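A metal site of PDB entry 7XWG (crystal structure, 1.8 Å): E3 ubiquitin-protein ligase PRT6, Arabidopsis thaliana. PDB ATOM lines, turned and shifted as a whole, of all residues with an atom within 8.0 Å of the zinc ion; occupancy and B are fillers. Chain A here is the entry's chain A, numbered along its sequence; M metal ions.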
ATOM      1  N   ARG A  21      -4.714  -5.267   5.638  1.00  0.00           N
ATOM      2  CA  ARG A  21      -5.834  -4.475   6.141  1.00  0.00           C
ATOM      3  C   ARG A  21      -6.844  -4.355   5.008  1.00  0.00           C
ATOM      4  O   ARG A  21      -6.444  -4.129   3.858  1.00  0.00           O
ATOM      5  CB  ARG A  21      -5.364  -3.088   6.585  1.00  0.00           C
ATOM      6  CG  ARG A  21      -6.508  -2.116   6.834  1.00  0.00           C
ATOM      7  CD  ARG A  21      -6.081  -0.888   7.570  1.00  0.00           C
ATOM      8  NE  ARG A  21      -7.279  -0.192   8.036  1.00  0.00           N
ATOM      9  CZ  ARG A  21      -7.319   1.099   8.343  1.00  0.00           C
ATOM     10  NH1 ARG A  21      -6.244   1.848   8.253  1.00  0.00           N
ATOM     11  NH2 ARG A  21      -8.455   1.632   8.728  1.00  0.00           N
ATOM     12  N   CYS A  22      -8.143  -4.476   5.298  1.00  0.00           N
ATOM     13  CA  CYS A  22      -9.157  -4.130   4.297  1.00  0.00           C
ATOM     14  C   CYS A  22     -10.173  -3.220   4.965  1.00  0.00           C
ATOM     15  O   CYS A  22     -10.947  -3.696   5.818  1.00  0.00           O
ATOM     16  CB  CYS A  22      -9.827  -5.383   3.701  1.00  0.00           C
ATOM     17  SG  CYS A  22     -11.097  -5.021   2.503  1.00  0.00           S
ATOM     18  N   ARG A  23     -10.188  -1.967   4.531  1.00  0.00           N
ATOM     19  CA  ARG A  23     -11.093  -1.004   5.161  1.00  0.00           C
ATOM     20  C   ARG A  23     -12.577  -1.299   4.876  1.00  0.00           C
ATOM     21  O   ARG A  23     -13.450  -0.865   5.623  1.00  0.00           O
ATOM     22  CB  ARG A  23     -10.719   0.413   4.719  1.00  0.00           C
ATOM     23  CG  ARG A  23      -9.265   0.768   5.099  1.00  0.00           C
ATOM     24  CD  ARG A  23      -8.731   2.021   4.419  1.00  0.00           C
ATOM     25  NE  ARG A  23      -7.323   2.280   4.724  1.00  0.00           N
ATOM     26  CZ  ARG A  23      -6.307   1.581   4.211  1.00  0.00           C
ATOM     27  NH1 ARG A  23      -6.536   0.598   3.364  1.00  0.00           N
ATOM     28  NH2 ARG A  23      -5.049   1.879   4.534  1.00  0.00           N
ATOM     29  N   THR A  24     -12.861  -2.025   3.823  1.00  0.00           N
ATOM     30  CA  THR A  24     -14.238  -2.379   3.519  1.00  0.00           C
ATOM     31  C   THR A  24     -14.761  -3.454   4.476  1.00  0.00           C
ATOM     32  O   THR A  24     -15.904  -3.387   4.931  1.00  0.00           O
ATOM     33  CB  THR A  24     -14.312  -2.864   2.072  1.00  0.00           C
ATOM     34  OG1 THR A  24     -13.613  -1.926   1.268  1.00  0.00           O
ATOM     35  CG2 THR A  24     -15.722  -3.029   1.574  1.00  0.00           C
ATOM     36  N   CYS A  25     -13.912  -4.435   4.801  1.00  0.00           N
ATOM     37  CA  CYS A  25     -14.359  -5.590   5.568  1.00  0.00           C
ATOM     38  C   CYS A  25     -14.127  -5.432   7.063  1.00  0.00           C
ATOM     39  O   CYS A  25     -14.765  -6.131   7.855  1.00  0.00           O
ATOM     40  CB  CYS A  25     -13.627  -6.850   5.078  1.00  0.00           C
ATOM     41  SG  CYS A  25     -14.053  -7.368   3.388  1.00  0.00           S
ATOM     42  N   GLU A  26     -13.213  -4.571   7.465  1.00  0.00           N
ATOM     43  CA  GLU A  26     -12.797  -4.449   8.880  1.00  0.00           C
ATOM     44  C   GLU A  26     -13.914  -3.917   9.781  1.00  0.00           C
ATOM     45  O   GLU A  26     -14.667  -3.112   9.329  1.00  0.00           O
ATOM     46  CB  GLU A  26     -11.570  -3.569   8.976  1.00  0.00           C
ATOM     47  CG  GLU A  26     -11.845  -2.089   8.927  1.00  0.00           C
ATOM     48  CD  GLU A  26     -10.585  -1.264   8.872  1.00  0.00           C
ATOM     49  OE1 GLU A  26      -9.555  -1.825   8.686  1.00  0.00           O
ATOM     50  OE2 GLU A  26     -10.660  -0.107   9.029  1.00  0.00           O
ATOM     51  N   ILE A  33      -6.187  -9.583   8.300  1.00  0.00           N
ATOM     52  CA  ILE A  33      -6.191 -11.010   7.968  1.00  0.00           C
ATOM     53  C   ILE A  33      -4.870 -11.390   7.304  1.00  0.00           C
ATOM     54  O   ILE A  33      -4.185 -10.540   6.733  1.00  0.00           O
ATOM     55  CB  ILE A  33      -7.368 -11.366   7.036  1.00  0.00           C
ATOM     56  CG1 ILE A  33      -7.285 -10.578   5.741  1.00  0.00           C
ATOM     57  CG2 ILE A  33      -8.683 -11.023   7.726  1.00  0.00           C
ATOM     58  CD1 ILE A  33      -8.332 -11.009   4.693  1.00  0.00           C
ATOM     59  N   PHE A  38      -6.591 -13.501   2.754  1.00  0.00           N
ATOM     60  CA  PHE A  38      -6.898 -12.457   1.777  1.00  0.00           C
ATOM     61  C   PHE A  38      -6.934 -13.020   0.358  1.00  0.00           C
ATOM     62  O   PHE A  38      -7.856 -12.728  -0.410  1.00  0.00           O
ATOM     63  CB  PHE A  38      -5.891 -11.321   1.889  1.00  0.00           C
ATOM     64  CG  PHE A  38      -6.157 -10.181   0.943  1.00  0.00           C
ATOM     65  CD1 PHE A  38      -6.952  -9.109   1.326  1.00  0.00           C
ATOM     66  CD2 PHE A  38      -5.631 -10.196  -0.337  1.00  0.00           C
ATOM     67  CE1 PHE A  38      -7.199  -8.090   0.469  1.00  0.00           C
ATOM     68  CE2 PHE A  38      -5.892  -9.167  -1.211  1.00  0.00           C
ATOM     69  CZ  PHE A  38      -6.672  -8.112  -0.799  1.00  0.00           C
ATOM     70  N   GLY A  41     -10.102 -14.915  -0.585  1.00  0.00           N
ATOM     71  CA  GLY A  41     -11.349 -14.190  -0.537  1.00  0.00           C
ATOM     72  C   GLY A  41     -11.445 -13.287  -1.735  1.00  0.00           C
ATOM     73  O   GLY A  41     -10.583 -13.323  -2.610  1.00  0.00           O
ATOM     74  N   ASP A  42     -12.463 -12.446  -1.756  1.00  0.00           N
ATOM     75  CA  ASP A  42     -12.716 -11.525  -2.873  1.00  0.00           C
ATOM     76  C   ASP A  42     -12.777 -10.116  -2.308  1.00  0.00           C
ATOM     77  O   ASP A  42     -13.765  -9.762  -1.649  1.00  0.00           O
ATOM     78  CB  ASP A  42     -14.009 -11.922  -3.588  1.00  0.00           C
ATOM     79  CG  ASP A  42     -14.399 -10.963  -4.714  1.00  0.00           C
ATOM     80  OD1 ASP A  42     -13.502 -10.334  -5.303  1.00  0.00           O
ATOM     81  OD2 ASP A  42     -15.610 -10.859  -5.026  1.00  0.00           O
ATOM     82  N   HIS A  43     -11.733  -9.320  -2.558  1.00  0.00           N
ATOM     83  CA  HIS A  43     -11.682  -7.922  -2.132  1.00  0.00           C
ATOM     84  C   HIS A  43     -11.429  -6.976  -3.310  1.00  0.00           C
ATOM     85  O   HIS A  43     -10.925  -5.881  -3.113  1.00  0.00           O
ATOM     86  CB  HIS A  43     -10.601  -7.734  -1.061  1.00  0.00           C
ATOM     87  CG  HIS A  43     -10.761  -8.675   0.084  1.00  0.00           C
ATOM     88  ND1 HIS A  43     -11.361  -8.300   1.261  1.00  0.00           N
ATOM     89  CD2 HIS A  43     -10.466  -9.986   0.208  1.00  0.00           C
ATOM     90  CE1 HIS A  43     -11.438  -9.348   2.062  1.00  0.00           C
ATOM     91  NE2 HIS A  43     -10.874 -10.376   1.456  1.00  0.00           N
ATOM     92  N   ASN A  44     -11.770  -7.385  -4.523  1.00  0.00           N
ATOM     93  CA  ASN A  44     -11.268  -6.676  -5.699  1.00  0.00           C
ATOM     94  C   ASN A  44     -11.625  -5.190  -5.668  1.00  0.00           C
ATOM     95  O   ASN A  44     -10.773  -4.324  -5.951  1.00  0.00           O
ATOM     96  CB  ASN A  44     -11.782  -7.364  -6.964  1.00  0.00           C
ATOM     97  CG  ASN A  44     -11.056  -8.678  -7.208  1.00  0.00           C
ATOM     98  OD1 ASN A  44      -9.894  -8.849  -6.806  1.00  0.00           O
ATOM     99  ND2 ASN A  44     -11.732  -9.611  -7.865  1.00  0.00           N
ATOM    100  N   SER A  45     -12.849  -4.865  -5.341  1.00  0.00           N
ATOM    101  CA  SER A  45     -13.261  -3.469  -5.268  1.00  0.00           C
ATOM    102  C   SER A  45     -12.876  -2.795  -3.963  1.00  0.00           C
ATOM    103  O   SER A  45     -13.203  -1.613  -3.795  1.00  0.00           O
ATOM    104  CB  SER A  45     -14.764  -3.380  -5.452  1.00  0.00           C
ATOM    105  OG  SER A  45     -15.414  -4.373  -4.673  1.00  0.00           O
ATOM    106  N   HIS A  46     -12.314  -3.518  -3.001  1.00  0.00           N
ATOM    107  CA  HIS A  46     -12.264  -3.032  -1.644  1.00  0.00           C
ATOM    108  C   HIS A  46     -11.059  -2.113  -1.442  1.00  0.00           C
ATOM    109  O   HIS A  46     -10.111  -2.129  -2.239  1.00  0.00           O
ATOM    110  CB  HIS A  46     -12.184  -4.190  -0.653  1.00  0.00           C
ATOM    111  CG  HIS A  46     -13.381  -5.098  -0.670  1.00  0.00           C
ATOM    112  ND1 HIS A  46     -13.585  -6.058   0.298  1.00  0.00           N
ATOM    113  CD2 HIS A  46     -14.418  -5.206  -1.541  1.00  0.00           C
ATOM    114  CE1 HIS A  46     -14.710  -6.703   0.037  1.00  0.00           C
ATOM    115  NE2 HIS A  46     -15.228  -6.216  -1.085  1.00  0.00           N
ATOM    116  N   ASP A  47     -11.090  -1.347  -0.350  1.00  0.00           N
ATOM    117  CA  ASP A  47      -9.978  -0.445  -0.046  1.00  0.00           C
ATOM    118  C   ASP A  47      -9.011  -1.183   0.874  1.00  0.00           C
ATOM    119  O   ASP A  47      -9.042  -1.062   2.096  1.00  0.00           O
ATOM    120  CB  ASP A  47     -10.498   0.852   0.561  1.00  0.00           C
ATOM    121  CG  ASP A  47      -9.406   1.886   0.673  1.00  0.00           C
ATOM    122  OD1 ASP A  47      -8.264   1.549   0.331  1.00  0.00           O
ATOM    123  OD2 ASP A  47      -9.654   3.012   1.127  1.00  0.00           O
ATOM    124  N   TYR A  48      -8.130  -1.971   0.259  1.00  0.00           N
ATOM    125  CA  TYR A  48      -7.211  -2.808   1.018  1.00  0.00           C
ATOM    126  C   TYR A  48      -5.778  -2.321   0.883  1.00  0.00           C
ATOM    127  O   TYR A  48      -5.444  -1.569  -0.032  1.00  0.00           O
ATOM    128  CB  TYR A  48      -7.297  -4.277   0.610  1.00  0.00           C
ATOM    129  CG  TYR A  48      -6.980  -4.568  -0.818  1.00  0.00           C
ATOM    130  CD1 TYR A  48      -5.667  -4.729  -1.236  1.00  0.00           C
ATOM    131  CD2 TYR A  48      -7.978  -4.708  -1.757  1.00  0.00           C
ATOM    132  CE1 TYR A  48      -5.368  -5.011  -2.544  1.00  0.00           C
ATOM    133  CE2 TYR A  48      -7.690  -4.978  -3.074  1.00  0.00           C
ATOM    134  CZ  TYR A  48      -6.374  -5.117  -3.452  1.00  0.00           C
ATOM    135  OH  TYR A  48      -6.048  -5.386  -4.764  1.00  0.00           O
ATOM    136  N   TRP A  66     -14.553  -8.945  11.457  1.00  0.00           N
ATOM    137  CA  TRP A  66     -14.508  -8.978  10.002  1.00  0.00           C
ATOM    138  C   TRP A  66     -15.893  -9.295   9.495  1.00  0.00           C
ATOM    139  O   TRP A  66     -16.546 -10.175  10.034  1.00  0.00           O
ATOM    140  CB  TRP A  66     -13.573 -10.067   9.524  1.00  0.00           C
ATOM    141  CG  TRP A  66     -12.886  -9.827   8.238  1.00  0.00           C
ATOM    142  CD1 TRP A  66     -13.147 -10.443   7.067  1.00  0.00           C
ATOM    143  CD2 TRP A  66     -11.780  -8.940   7.988  1.00  0.00           C
ATOM    144  NE1 TRP A  66     -12.294  -9.995   6.093  1.00  0.00           N
ATOM    145  CE2 TRP A  66     -11.438  -9.074   6.635  1.00  0.00           C
ATOM    146  CE3 TRP A  66     -11.067  -8.042   8.779  1.00  0.00           C
ATOM    147  CZ2 TRP A  66     -10.398  -8.348   6.042  1.00  0.00           C
ATOM    148  CZ3 TRP A  66     -10.020  -7.306   8.192  1.00  0.00           C
ATOM    149  CH2 TRP A  66      -9.694  -7.471   6.829  1.00  0.00           C
ATOM    150  N   LYS A  67     -16.265  -8.633   8.410  1.00  0.00           N
ATOM    151  CA  LYS A  67     -17.559  -8.869   7.758  1.00  0.00           C
ATOM    152  C   LYS A  67     -17.552 -10.235   7.066  1.00  0.00           C
ATOM    153  O   LYS A  67     -16.580 -10.572   6.379  1.00  0.00           O
ATOM    154  CB  LYS A  67     -17.856  -7.787   6.736  1.00  0.00           C
ATOM    155  CG  LYS A  67     -18.247  -6.474   7.415  1.00  0.00           C
ATOM    156  CD  LYS A  67     -18.249  -5.312   6.443  1.00  0.00           C
ATOM    157  CE  LYS A  67     -18.577  -4.003   7.171  1.00  0.00           C
ATOM    158  NZ  LYS A  67     -17.397  -3.118   7.345  1.00  0.00           N
ATOM    159  N   ASP A  69     -18.904 -11.233   4.392  1.00  0.00           N
ATOM    160  CA  ASP A  69     -18.608 -11.081   2.968  1.00  0.00           C
ATOM    161  C   ASP A  69     -17.116 -11.129   2.705  1.00  0.00           C
ATOM    162  O   ASP A  69     -16.705 -11.445   1.572  1.00  0.00           O
ATOM    163  CB  ASP A  69     -19.204  -9.764   2.459  1.00  0.00           C
ATOM    164  CG  ASP A  69     -18.899  -9.512   0.981  1.00  0.00           C
ATOM    165  OD1 ASP A  69     -19.546 -10.165   0.130  1.00  0.00           O
ATOM    166  OD2 ASP A  69     -18.025  -8.665   0.657  1.00  0.00           O
ATOM    167  N   GLY A  70     -16.312 -10.832   3.720  1.00  0.00           N
ATOM    168  CA  GLY A  70     -14.872 -10.802   3.590  1.00  0.00           C
ATOM    169  C   GLY A  70     -14.157 -12.032   4.074  1.00  0.00           C
ATOM    170  O   GLY A  70     -12.914 -12.087   4.006  1.00  0.00           O
ATOM    171  N   PHE A  71     -14.884 -13.044   4.536  1.00  0.00           N
ATOM    172  CA  PHE A  71     -14.275 -14.309   4.907  1.00  0.00           C
ATOM    173  C   PHE A  71     -13.699 -14.996   3.682  1.00  0.00           C
ATOM    174  O   PHE A  71     -14.265 -14.922   2.583  1.00  0.00           O
ATOM    175  CB  PHE A  71     -15.311 -15.230   5.543  1.00  0.00           C
ATOM    176  CG  PHE A  71     -15.821 -14.758   6.874  1.00  0.00           C
ATOM    177  CD1 PHE A  71     -16.890 -15.420   7.470  1.00  0.00           C
ATOM    178  CD2 PHE A  71     -15.251 -13.687   7.524  1.00  0.00           C
ATOM    179  CE1 PHE A  71     -17.385 -15.015   8.705  1.00  0.00           C
ATOM    180  CE2 PHE A  71     -15.717 -13.285   8.779  1.00  0.00           C
ATOM    181  CZ  PHE A  71     -16.794 -13.949   9.358  1.00  0.00           C
HETATM  182 ZN    ZN M   1     -12.396  -6.703   1.881  1.00  0.00          ZN
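The side-chain sulfur (SG) of Cys 22 lies close to the backbone NH (N) of Thr 24.
O of Cys 25 is in hydrogen-bond range of N of Lys 67, 3.0 Å away.
The zinc ion is bound by ND1 of His 43 (2.0 Å), ND1 of His 46 (2.1 Å), SG of Cys 22 (2.2 Å) and SG of Cys 25 (2.3 Å).
Of the 21 residues printed, 4 come within 4 Å of the zinc ion.
The nearest printed residue that does not touch the zinc ion is Thr 24 (4.3 Å).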
